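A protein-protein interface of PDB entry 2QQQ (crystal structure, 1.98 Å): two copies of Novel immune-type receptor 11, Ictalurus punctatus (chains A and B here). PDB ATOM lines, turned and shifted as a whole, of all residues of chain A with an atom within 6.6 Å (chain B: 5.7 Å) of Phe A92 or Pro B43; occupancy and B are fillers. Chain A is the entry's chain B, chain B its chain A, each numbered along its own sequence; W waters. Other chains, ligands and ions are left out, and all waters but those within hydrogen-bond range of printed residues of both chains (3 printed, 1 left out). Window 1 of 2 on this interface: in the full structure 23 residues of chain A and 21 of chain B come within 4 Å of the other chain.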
ATOM      1  N   LYS A   4      16.757  35.775  27.841  1.00  0.00           N
ATOM      2  CA  LYS A   4      15.440  35.138  28.011  1.00  0.00           C
ATOM      3  C   LYS A   4      15.579  33.849  28.826  1.00  0.00           C
ATOM      4  O   LYS A   4      16.354  32.953  28.466  1.00  0.00           O
ATOM      5  CB  LYS A   4      14.824  34.854  26.629  1.00  0.00           C
ATOM      6  CG  LYS A   4      13.435  34.300  26.638  1.00  0.00           C
ATOM      7  CD  LYS A   4      12.445  35.277  27.294  1.00  0.00           C
ATOM      8  CE  LYS A   4      11.061  34.647  27.457  1.00  0.00           C
ATOM      9  NZ  LYS A   4      10.746  33.660  26.382  1.00  0.00           N
ATOM     10  N   LEU A   6      14.540  30.148  30.233  1.00  0.00           N
ATOM     11  CA  LEU A   6      13.751  28.983  29.930  1.00  0.00           C
ATOM     12  C   LEU A   6      12.661  28.797  30.981  1.00  0.00           C
ATOM     13  O   LEU A   6      12.917  28.928  32.156  1.00  0.00           O
ATOM     14  CB  LEU A   6      14.608  27.678  29.956  1.00  0.00           C
ATOM     15  CG  LEU A   6      15.914  27.664  29.104  1.00  0.00           C
ATOM     16  CD1 LEU A   6      16.654  26.400  29.218  1.00  0.00           C
ATOM     17  CD2 LEU A   6      15.469  27.862  27.707  1.00  0.00           C
ATOM     18  N   ALA A  33      11.115  27.555  14.000  1.00  0.00           N
ATOM     19  CA  ALA A  33      11.404  26.144  14.247  1.00  0.00           C
ATOM     20  C   ALA A  33      11.726  25.890  15.696  1.00  0.00           C
ATOM     21  O   ALA A  33      12.270  26.766  16.355  1.00  0.00           O
ATOM     22  CB  ALA A  33      12.620  25.646  13.276  1.00  0.00           C
ATOM     23  N   TRP A  34      11.326  24.732  16.219  1.00  0.00           N
ATOM     24  CA  TRP A  34      11.778  24.255  17.514  1.00  0.00           C
ATOM     25  C   TRP A  34      13.039  23.386  17.284  1.00  0.00           C
ATOM     26  O   TRP A  34      13.112  22.638  16.279  1.00  0.00           O
ATOM     27  CB  TRP A  34      10.723  23.357  18.196  1.00  0.00           C
ATOM     28  CG  TRP A  34       9.601  24.152  18.891  1.00  0.00           C
ATOM     29  CD1 TRP A  34       8.405  24.509  18.364  1.00  0.00           C
ATOM     30  CD2 TRP A  34       9.645  24.700  20.219  1.00  0.00           C
ATOM     31  NE1 TRP A  34       7.674  25.229  19.299  1.00  0.00           N
ATOM     32  CE2 TRP A  34       8.410  25.330  20.453  1.00  0.00           C
ATOM     33  CE3 TRP A  34      10.594  24.661  21.262  1.00  0.00           C
ATOM     34  CZ2 TRP A  34       8.120  25.979  21.657  1.00  0.00           C
ATOM     35  CZ3 TRP A  34      10.278  25.289  22.488  1.00  0.00           C
ATOM     36  CH2 TRP A  34       9.057  25.932  22.655  1.00  0.00           C
ATOM     37  N   TYR A  35      13.968  23.488  18.254  1.00  0.00           N
ATOM     38  CA  TYR A  35      15.157  22.657  18.377  1.00  0.00           C
ATOM     39  C   TYR A  35      15.024  21.887  19.683  1.00  0.00           C
ATOM     40  O   TYR A  35      14.463  22.395  20.657  1.00  0.00           O
ATOM     41  CB  TYR A  35      16.416  23.532  18.356  1.00  0.00           C
ATOM     42  CG  TYR A  35      16.706  24.055  16.953  1.00  0.00           C
ATOM     43  CD1 TYR A  35      15.922  25.064  16.350  1.00  0.00           C
ATOM     44  CD2 TYR A  35      17.753  23.495  16.199  1.00  0.00           C
ATOM     45  CE1 TYR A  35      16.202  25.489  15.031  1.00  0.00           C
ATOM     46  CE2 TYR A  35      18.035  23.917  14.932  1.00  0.00           C
ATOM     47  CZ  TYR A  35      17.257  24.886  14.345  1.00  0.00           C
ATOM     48  OH  TYR A  35      17.604  25.232  13.059  1.00  0.00           O
ATOM     49  N   ARG A  36      15.557  20.657  19.731  1.00  0.00           N
ATOM     50  CA  ARG A  36      15.445  19.816  20.949  1.00  0.00           C
ATOM     51  C   ARG A  36      16.863  19.376  21.326  1.00  0.00           C
ATOM     52  O   ARG A  36      17.650  18.909  20.476  1.00  0.00           O
ATOM     53  CB  ARG A  36      14.536  18.620  20.654  1.00  0.00           C
ATOM     54  CG  ARG A  36      14.504  17.524  21.742  1.00  0.00           C
ATOM     55  CD  ARG A  36      13.708  16.346  21.251  1.00  0.00           C
ATOM     56  NE  ARG A  36      13.748  15.259  22.227  1.00  0.00           N
ATOM     57  CZ  ARG A  36      12.972  14.187  22.173  1.00  0.00           C
ATOM     58  NH1 ARG A  36      12.051  14.069  21.208  1.00  0.00           N
ATOM     59  NH2 ARG A  36      13.094  13.246  23.103  1.00  0.00           N
ATOM     60  N   GLN A  37      17.197  19.626  22.571  1.00  0.00           N
ATOM     61  CA  GLN A  37      18.434  19.221  23.144  1.00  0.00           C
ATOM     62  C   GLN A  37      18.281  18.207  24.275  1.00  0.00           C
ATOM     63  O   GLN A  37      17.890  18.545  25.419  1.00  0.00           O
ATOM     64  CB  GLN A  37      19.208  20.429  23.633  1.00  0.00           C
ATOM     65  CG  GLN A  37      20.555  19.991  24.195  1.00  0.00           C
ATOM     66  CD  GLN A  37      21.336  21.059  24.845  1.00  0.00           C
ATOM     67  OE1 GLN A  37      20.790  22.099  25.321  1.00  0.00           O
ATOM     68  NE2 GLN A  37      22.642  20.816  24.933  1.00  0.00           N
ATOM     69  N   PRO A  43      22.094  20.316  20.363  1.00  0.00           N
ATOM     70  CA  PRO A  43      20.717  20.532  19.910  1.00  0.00           C
ATOM     71  C   PRO A  43      20.556  20.116  18.459  1.00  0.00           C
ATOM     72  O   PRO A  43      21.535  20.167  17.674  1.00  0.00           O
ATOM     73  CB  PRO A  43      20.509  22.047  20.014  1.00  0.00           C
ATOM     74  CG  PRO A  43      21.606  22.512  20.999  1.00  0.00           C
ATOM     75  CD  PRO A  43      22.736  21.556  20.843  1.00  0.00           C
ATOM     76  N   GLU A  90      15.896  20.014  26.832  1.00  0.00           N
ATOM     77  CA  GLU A  90      15.596  21.437  26.602  1.00  0.00           C
ATOM     78  C   GLU A  90      15.156  21.585  25.184  1.00  0.00           C
ATOM     79  O   GLU A  90      15.694  20.890  24.231  1.00  0.00           O
ATOM     80  CB  GLU A  90      16.798  22.363  26.920  1.00  0.00           C
ATOM     81  CG  GLU A  90      17.459  22.043  28.225  1.00  0.00           C
ATOM     82  CD  GLU A  90      18.527  23.047  28.660  1.00  0.00           C
ATOM     83  OE1 GLU A  90      18.676  23.288  29.883  1.00  0.00           O
ATOM     84  OE2 GLU A  90      19.160  23.632  27.809  1.00  0.00           O
ATOM     85  N   TYR A  91      14.160  22.461  25.034  1.00  0.00           N
ATOM     86  CA  TYR A  91      13.510  22.715  23.768  1.00  0.00           C
ATOM     87  C   TYR A  91      13.563  24.202  23.582  1.00  0.00           C
ATOM     88  O   TYR A  91      13.196  24.960  24.479  1.00  0.00           O
ATOM     89  CB  TYR A  91      12.019  22.266  23.818  1.00  0.00           C
ATOM     90  CG  TYR A  91      11.851  20.773  23.956  1.00  0.00           C
ATOM     91  CD1 TYR A  91      12.008  20.150  25.194  1.00  0.00           C
ATOM     92  CD2 TYR A  91      11.589  19.987  22.843  1.00  0.00           C
ATOM     93  CE1 TYR A  91      11.945  18.733  25.306  1.00  0.00           C
ATOM     94  CE2 TYR A  91      11.457  18.580  22.947  1.00  0.00           C
ATOM     95  CZ  TYR A  91      11.629  17.976  24.180  1.00  0.00           C
ATOM     96  OH  TYR A  91      11.476  16.632  24.251  1.00  0.00           O
ATOM     97  N   PHE A  92      14.034  24.637  22.426  1.00  0.00           N
ATOM     98  CA  PHE A  92      14.205  26.078  22.146  1.00  0.00           C
ATOM     99  C   PHE A  92      13.536  26.424  20.865  1.00  0.00           C
ATOM    100  O   PHE A  92      13.699  25.708  19.910  1.00  0.00           O
ATOM    101  CB  PHE A  92      15.643  26.536  22.015  1.00  0.00           C
ATOM    102  CG  PHE A  92      16.582  25.862  22.915  1.00  0.00           C
ATOM    103  CD1 PHE A  92      17.563  24.982  22.404  1.00  0.00           C
ATOM    104  CD2 PHE A  92      16.522  26.050  24.264  1.00  0.00           C
ATOM    105  CE1 PHE A  92      18.487  24.374  23.276  1.00  0.00           C
ATOM    106  CE2 PHE A  92      17.415  25.404  25.134  1.00  0.00           C
ATOM    107  CZ  PHE A  92      18.427  24.565  24.609  1.00  0.00           C
ATOM    108  N   CYS A  93      12.815  27.539  20.865  1.00  0.00           N
ATOM    109  CA  CYS A  93      12.057  28.009  19.687  1.00  0.00           C
ATOM    110  C   CYS A  93      12.710  29.243  19.123  1.00  0.00           C
ATOM    111  O   CYS A  93      12.916  30.215  19.848  1.00  0.00           O
ATOM    112  CB  CYS A  93      10.589  28.354  20.065  1.00  0.00           C
ATOM    113  SG  CYS A  93       9.569  28.772  18.661  1.00  0.00           S
ATOM    114  N   GLY A  94      13.039  29.205  17.829  1.00  0.00           N
ATOM    115  CA  GLY A  94      13.769  30.289  17.225  1.00  0.00           C
ATOM    116  C   GLY A  94      13.502  30.544  15.788  1.00  0.00           C
ATOM    117  O   GLY A  94      13.121  29.687  15.042  1.00  0.00           O
ATOM    118  N   ILE A 101      20.234  32.428  14.025  1.00  0.00           N
ATOM    119  CA  ILE A 101      18.992  31.974  14.639  1.00  0.00           C
ATOM    120  C   ILE A 101      18.792  32.777  15.944  1.00  0.00           C
ATOM    121  O   ILE A 101      19.701  32.897  16.712  1.00  0.00           O
ATOM    122  CB  ILE A 101      18.968  30.400  14.826  1.00  0.00           C
ATOM    123  CG1 ILE A 101      17.594  29.875  15.268  1.00  0.00           C
ATOM    124  CG2 ILE A 101      20.026  29.881  15.727  1.00  0.00           C
ATOM    125  CD1 ILE A 101      17.056  30.348  16.638  1.00  0.00           C
ATOM    126  N   LYS A 102      17.620  33.387  16.149  1.00  0.00           N
ATOM    127  CA  LYS A 102      17.311  34.014  17.434  1.00  0.00           C
ATOM    128  C   LYS A 102      16.311  33.153  18.124  1.00  0.00           C
ATOM    129  O   LYS A 102      15.245  32.876  17.555  1.00  0.00           O
ATOM    130  CB  LYS A 102      16.671  35.393  17.265  1.00  0.00           C
ATOM    131  CG  LYS A 102      17.621  36.511  17.102  1.00  0.00           C
ATOM    132  CD  LYS A 102      18.202  36.991  18.463  1.00  0.00           C
ATOM    133  CE  LYS A 102      19.437  37.916  18.298  1.00  0.00           C
ATOM    134  NZ  LYS A 102      19.221  39.002  17.262  1.00  0.00           N
ATOM    135  N   PHE A 103      16.634  32.740  19.351  1.00  0.00           N
ATOM    136  CA  PHE A 103      15.785  31.858  20.107  1.00  0.00           C
ATOM    137  C   PHE A 103      14.918  32.739  21.009  1.00  0.00           C
ATOM    138  O   PHE A 103      15.436  33.559  21.770  1.00  0.00           O
ATOM    139  CB  PHE A 103      16.627  30.834  20.902  1.00  0.00           C
ATOM    140  CG  PHE A 103      17.270  29.761  20.042  1.00  0.00           C
ATOM    141  CD1 PHE A 103      16.503  28.759  19.479  1.00  0.00           C
ATOM    142  CD2 PHE A 103      18.647  29.763  19.813  1.00  0.00           C
ATOM    143  CE1 PHE A 103      17.060  27.730  18.653  1.00  0.00           C
ATOM    144  CE2 PHE A 103      19.225  28.756  19.013  1.00  0.00           C
ATOM    145  CZ  PHE A 103      18.446  27.741  18.455  1.00  0.00           C
ATOM    146  N   THR A 104      13.612  32.632  20.871  1.00  0.00           N
ATOM    147  CA  THR A 104      12.702  33.578  21.553  1.00  0.00           C
ATOM    148  C   THR A 104      12.110  33.070  22.849  1.00  0.00           C
ATOM    149  O   THR A 104      11.704  33.865  23.714  1.00  0.00           O
ATOM    150  CB  THR A 104      11.573  34.019  20.668  1.00  0.00           C
ATOM    151  OG1 THR A 104      10.861  32.863  20.177  1.00  0.00           O
ATOM    152  CG2 THR A 104      12.136  34.889  19.516  1.00  0.00           C
ATOM    153  N   SER A 105      12.096  31.749  23.002  1.00  0.00           N
ATOM    154  CA  SER A 105      11.707  31.114  24.249  1.00  0.00           C
ATOM    155  C   SER A 105      12.253  29.706  24.216  1.00  0.00           C
ATOM    156  O   SER A 105      12.656  29.212  23.172  1.00  0.00           O
ATOM    157  CB  SER A 105      10.172  31.048  24.405  1.00  0.00           C
ATOM    158  OG  SER A 105       9.600  30.397  23.298  1.00  0.00           O
ATOM    159  N   GLY A 106      12.236  29.093  25.382  1.00  0.00           N
ATOM    160  CA  GLY A 106      12.516  27.694  25.569  1.00  0.00           C
ATOM    161  C   GLY A 106      11.943  27.137  26.859  1.00  0.00           C
ATOM    162  O   GLY A 106      11.576  27.877  27.769  1.00  0.00           O
ATOM    163  N   THR A 107      11.908  25.813  26.925  1.00  0.00           N
ATOM    164  CA  THR A 107      11.404  25.042  28.086  1.00  0.00           C
ATOM    165  C   THR A 107      12.438  23.942  28.388  1.00  0.00           C
ATOM    166  O   THR A 107      12.936  23.293  27.468  1.00  0.00           O
ATOM    167  CB  THR A 107       9.982  24.429  27.781  1.00  0.00           C
ATOM    168  OG1 THR A 107       9.025  25.482  27.618  1.00  0.00           O
ATOM    169  CG2 THR A 107       9.438  23.597  28.918  1.00  0.00           C
ATOM    170  N   TYR B  35      27.301  29.509  19.344  1.00  0.00           N
ATOM    171  CA  TYR B  35      26.141  29.934  20.206  1.00  0.00           C
ATOM    172  C   TYR B  35      26.523  29.594  21.661  1.00  0.00           C
ATOM    173  O   TYR B  35      27.266  28.627  21.935  1.00  0.00           O
ATOM    174  CB  TYR B  35      24.836  29.200  19.745  1.00  0.00           C
ATOM    175  CG  TYR B  35      24.377  29.754  18.410  1.00  0.00           C
ATOM    176  CD1 TYR B  35      25.025  29.431  17.191  1.00  0.00           C
ATOM    177  CD2 TYR B  35      23.244  30.580  18.345  1.00  0.00           C
ATOM    178  CE1 TYR B  35      24.589  30.009  15.974  1.00  0.00           C
ATOM    179  CE2 TYR B  35      22.841  31.143  17.190  1.00  0.00           C
ATOM    180  CZ  TYR B  35      23.508  30.883  16.004  1.00  0.00           C
ATOM    181  OH  TYR B  35      23.023  31.517  14.891  1.00  0.00           O
ATOM    182  N   ARG B  36      26.058  30.417  22.601  1.00  0.00           N
ATOM    183  CA  ARG B  36      26.389  30.257  24.004  1.00  0.00           C
ATOM    184  C   ARG B  36      25.074  30.229  24.783  1.00  0.00           C
ATOM    185  O   ARG B  36      24.229  31.136  24.593  1.00  0.00           O
ATOM    186  CB  ARG B  36      27.244  31.447  24.462  1.00  0.00           C
ATOM    187  CG  ARG B  36      27.328  31.624  25.950  1.00  0.00           C
ATOM    188  CD  ARG B  36      28.315  32.747  26.280  1.00  0.00           C
ATOM    189  NE  ARG B  36      28.435  32.854  27.718  1.00  0.00           N
ATOM    190  CZ  ARG B  36      29.120  33.789  28.349  1.00  0.00           C
ATOM    191  NH1 ARG B  36      29.724  34.757  27.675  1.00  0.00           N
ATOM    192  NH2 ARG B  36      29.147  33.789  29.667  1.00  0.00           N
ATOM    193  N   GLN B  37      24.893  29.197  25.595  1.00  0.00           N
ATOM    194  CA  GLN B  37      23.731  29.076  26.452  1.00  0.00           C
ATOM    195  C   GLN B  37      24.131  28.974  27.944  1.00  0.00           C
ATOM    196  O   GLN B  37      24.710  27.970  28.364  1.00  0.00           O
ATOM    197  CB  GLN B  37      22.917  27.845  26.058  1.00  0.00           C
ATOM    198  CG  GLN B  37      21.660  27.711  26.844  1.00  0.00           C
ATOM    199  CD  GLN B  37      21.111  26.344  26.914  1.00  0.00           C
ATOM    200  OE1 GLN B  37      21.750  25.348  26.500  1.00  0.00           O
ATOM    201  NE2 GLN B  37      19.940  26.242  27.539  1.00  0.00           N
ATOM    202  N   LYS B  41      18.862  29.599  30.493  1.00  0.00           N
ATOM    203  CA  LYS B  41      18.558  30.680  29.564  1.00  0.00           C
ATOM    204  C   LYS B  41      18.475  30.055  28.165  1.00  0.00           C
ATOM    205  O   LYS B  41      18.953  28.980  27.945  1.00  0.00           O
ATOM    206  CB  LYS B  41      19.737  31.686  29.514  1.00  0.00           C
ATOM    207  CG  LYS B  41      20.126  32.446  30.801  1.00  0.00           C
ATOM    208  CD  LYS B  41      18.965  33.272  31.245  1.00  0.00           C
ATOM    209  CE  LYS B  41      19.449  34.455  32.024  1.00  0.00           C
ATOM    210  NZ  LYS B  41      19.832  33.970  33.332  1.00  0.00           N
ATOM    211  N   VAL B  42      17.919  30.779  27.225  1.00  0.00           N
ATOM    212  CA  VAL B  42      17.851  30.353  25.866  1.00  0.00           C
ATOM    213  C   VAL B  42      19.274  30.585  25.288  1.00  0.00           C
ATOM    214  O   VAL B  42      19.970  31.506  25.743  1.00  0.00           O
ATOM    215  CB  VAL B  42      16.728  31.229  25.217  1.00  0.00           C
ATOM    216  CG1 VAL B  42      17.265  32.381  24.477  1.00  0.00           C
ATOM    217  CG2 VAL B  42      15.805  30.404  24.406  1.00  0.00           C
ATOM    218  N   PRO B  43      19.718  29.736  24.322  1.00  0.00           N
ATOM    219  CA  PRO B  43      20.996  30.044  23.681  1.00  0.00           C
ATOM    220  C   PRO B  43      20.951  31.371  22.885  1.00  0.00           C
ATOM    221  O   PRO B  43      19.886  31.788  22.438  1.00  0.00           O
ATOM    222  CB  PRO B  43      21.193  28.891  22.665  1.00  0.00           C
ATOM    223  CG  PRO B  43      20.282  27.791  23.076  1.00  0.00           C
ATOM    224  CD  PRO B  43      19.112  28.487  23.799  1.00  0.00           C
ATOM    225  N   GLN B  44      22.145  31.946  22.652  1.00  0.00           N
ATOM    226  CA  GLN B  44      22.326  33.172  21.947  1.00  0.00           C
ATOM    227  C   GLN B  44      23.496  33.050  20.996  1.00  0.00           C
ATOM    228  O   GLN B  44      24.552  32.517  21.331  1.00  0.00           O
ATOM    229  CB  GLN B  44      22.585  34.268  22.945  1.00  0.00           C
ATOM    230  CG  GLN B  44      21.422  34.457  23.987  1.00  0.00           C
ATOM    231  CD  GLN B  44      20.356  35.369  23.485  1.00  0.00           C
ATOM    232  OE1 GLN B  44      20.627  36.273  22.667  1.00  0.00           O
ATOM    233  NE2 GLN B  44      19.121  35.169  23.972  1.00  0.00           N
ATOM    234  N   TYR B  45      23.255  33.516  19.782  1.00  0.00           N
ATOM    235  CA  TYR B  45      24.325  33.878  18.893  1.00  0.00           C
ATOM    236  C   TYR B  45      25.422  34.683  19.540  1.00  0.00           C
ATOM    237  O   TYR B  45      25.196  35.768  20.116  1.00  0.00           O
ATOM    238  CB  TYR B  45      23.759  34.639  17.693  1.00  0.00           C
ATOM    239  CG  TYR B  45      24.822  35.146  16.769  1.00  0.00           C
ATOM    240  CD1 TYR B  45      25.579  34.253  15.977  1.00  0.00           C
ATOM    241  CD2 TYR B  45      25.051  36.532  16.647  1.00  0.00           C
ATOM    242  CE1 TYR B  45      26.570  34.748  15.085  1.00  0.00           C
ATOM    243  CE2 TYR B  45      26.036  37.035  15.804  1.00  0.00           C
ATOM    244  CZ  TYR B  45      26.788  36.123  15.004  1.00  0.00           C
ATOM    245  OH  TYR B  45      27.755  36.660  14.143  1.00  0.00           O
ATOM    246  N   PHE B  92      27.770  25.876  21.443  1.00  0.00           N
ATOM    247  CA  PHE B  92      27.458  24.983  20.335  1.00  0.00           C
ATOM    248  C   PHE B  92      27.950  25.704  19.063  1.00  0.00           C
ATOM    249  O   PHE B  92      27.682  26.888  18.871  1.00  0.00           O
ATOM    250  CB  PHE B  92      25.969  24.761  20.177  1.00  0.00           C
ATOM    251  CG  PHE B  92      25.182  24.587  21.475  1.00  0.00           C
ATOM    252  CD1 PHE B  92      24.218  25.544  21.859  1.00  0.00           C
ATOM    253  CD2 PHE B  92      25.358  23.466  22.269  1.00  0.00           C
ATOM    254  CE1 PHE B  92      23.438  25.365  23.023  1.00  0.00           C
ATOM    255  CE2 PHE B  92      24.622  23.243  23.404  1.00  0.00           C
ATOM    256  CZ  PHE B  92      23.628  24.233  23.810  1.00  0.00           C
HETATM  257  O   HOH W   1      17.297  35.630  22.024  1.00  0.00           O
HETATM  258  O   HOH W   2      20.558  34.415  19.039  1.00  0.00           O
HETATM  259  O   HOH W   3      18.900  33.846  20.945  1.00  0.00           O
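The side-chain amide nitrogen (NE2) of Gln B37 is in hydrogen-bond range of the side-chain carboxylate (OE2) of Glu A90 (2.7 Å).
N of Val B42 is in hydrogen-bond range of O of Lys A4, 3.0 Å away.
The side-chain hydroxyl (OH) of Tyr B35 sits at hydrogen-bond distance from the backbone NH (N) of Ile A101 (3.1 Å).
N of Gln A37 is in hydrogen-bond range of O of Glu A90.
The backbone NH of Cys A93 lies within hydrogen-bond range of the backbone carbonyl oxygen of Ser A105, at 2.9 Å.
O of Phe B92 is in hydrogen-bond range of N of Tyr B35 (2.7 Å).
The backbone NH (N) of Tyr A35 lies within hydrogen-bond range of the backbone carbonyl oxygen (O) of Phe A92.
The side-chain amide nitrogen (NE2) of Gln B37 lies within hydrogen-bond range of the backbone carbonyl oxygen (O) of Lys B41, 2.9 Å away.
The backbone carbonyl oxygen of Thr A104 sits at hydrogen-bond distance from the side-chain amino group of Lys A4, 2.8 Å away.
Lys A4 touches Lys B41.
Leu A6 touches Lys B41.
Val B42 touches Leu A6.
Gln A37 touches Gln B37 (OE1 to OE1, 3.6 Å).
Pro A43 touches Phe B92 (CD to CD2, 3.5 Å).
Gln B37 touches Phe A92 (NE2 to CE2, 3.6 Å).
Phe A92 touches Pro B43 (CD2 to CD, 3.6 Å).
O of Phe A103 touches CG1 of Val B42, 3.5 Å away.
O of Pro B43 touches CD2 of Phe A103 (3.5 Å).
Gly A106 touches Val B42 (N to CG2, 3.9 Å).
Of the printed residues of chain B, Lys A4 touches Lys B41 (3.4 Å) and Val B42 (3.0 Å).
Of the printed residues of chain B, Glu A90 touches Gln B37 (2.7 Å).
Phe A92 touches just these residues of chain B: Gln B37 (3.6 Å) and Pro B43 (3.6 Å).
Of the printed residues of chain B, Ile A101 touches Tyr B35.
Pro B43 touches just these residues of chain A: Phe A92 and Phe A103.
The nearest residue of chain A that does not touch Pro B43 is Leu A6 (5.4 Å).
Of the 20 printed residues of chain A, 10 touch a printed residue of chain B.
Printed residues of chain B that touch a printed residue of chain A: Tyr B35, Gln B37, Lys B41, Val B42, Pro B43 and Phe B92.
Hydrophobic or aromatic side chains of chain B that line the printed part of chain A: Tyr B35, Val B42, Pro B43 and Phe B92.
Along chain B the printed residues that touch a printed residue of chain A span positions 35 to 92.
Among the printed residues, 16 pairs touch across the chains.
Among the printed residues, no Asp or Glu carboxylate lies within 4 Å of a Lys or Arg side-chain nitrogen of the other chain.
Gln A37 touches its own counterpart, Gln B37.
Gln A37 touches Phe B92, and with the chains exchanged Phe A92 touches Gln B37.
Pro A43 touches Phe B92, and with the chains exchanged Phe A92 touches Pro B43.
5 positions are printed for both chains.
Of the 16 pairs that touch across the chains among the printed residues, 5 have their exchanged pair printed and touching as well.
Water W1 lies within hydrogen-bond range of the side-chain amide nitrogen of Gln B44 (2.7 Å) and the backbone carbonyl oxygen of Phe A103 (2.8 Å).
Water W3 lies within hydrogen-bond range of the backbone carbonyl oxygen (O) of Pro B43 (2.7 Å), the backbone NH (N) of Phe A103 (3.0 Å) and the side-chain amide nitrogen (NE2) of Gln B44 (3.3 Å).
Water W2 lies within hydrogen-bond range of O of Ile A101 (2.9 Å) and N of Tyr B45 (2.9 Å).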
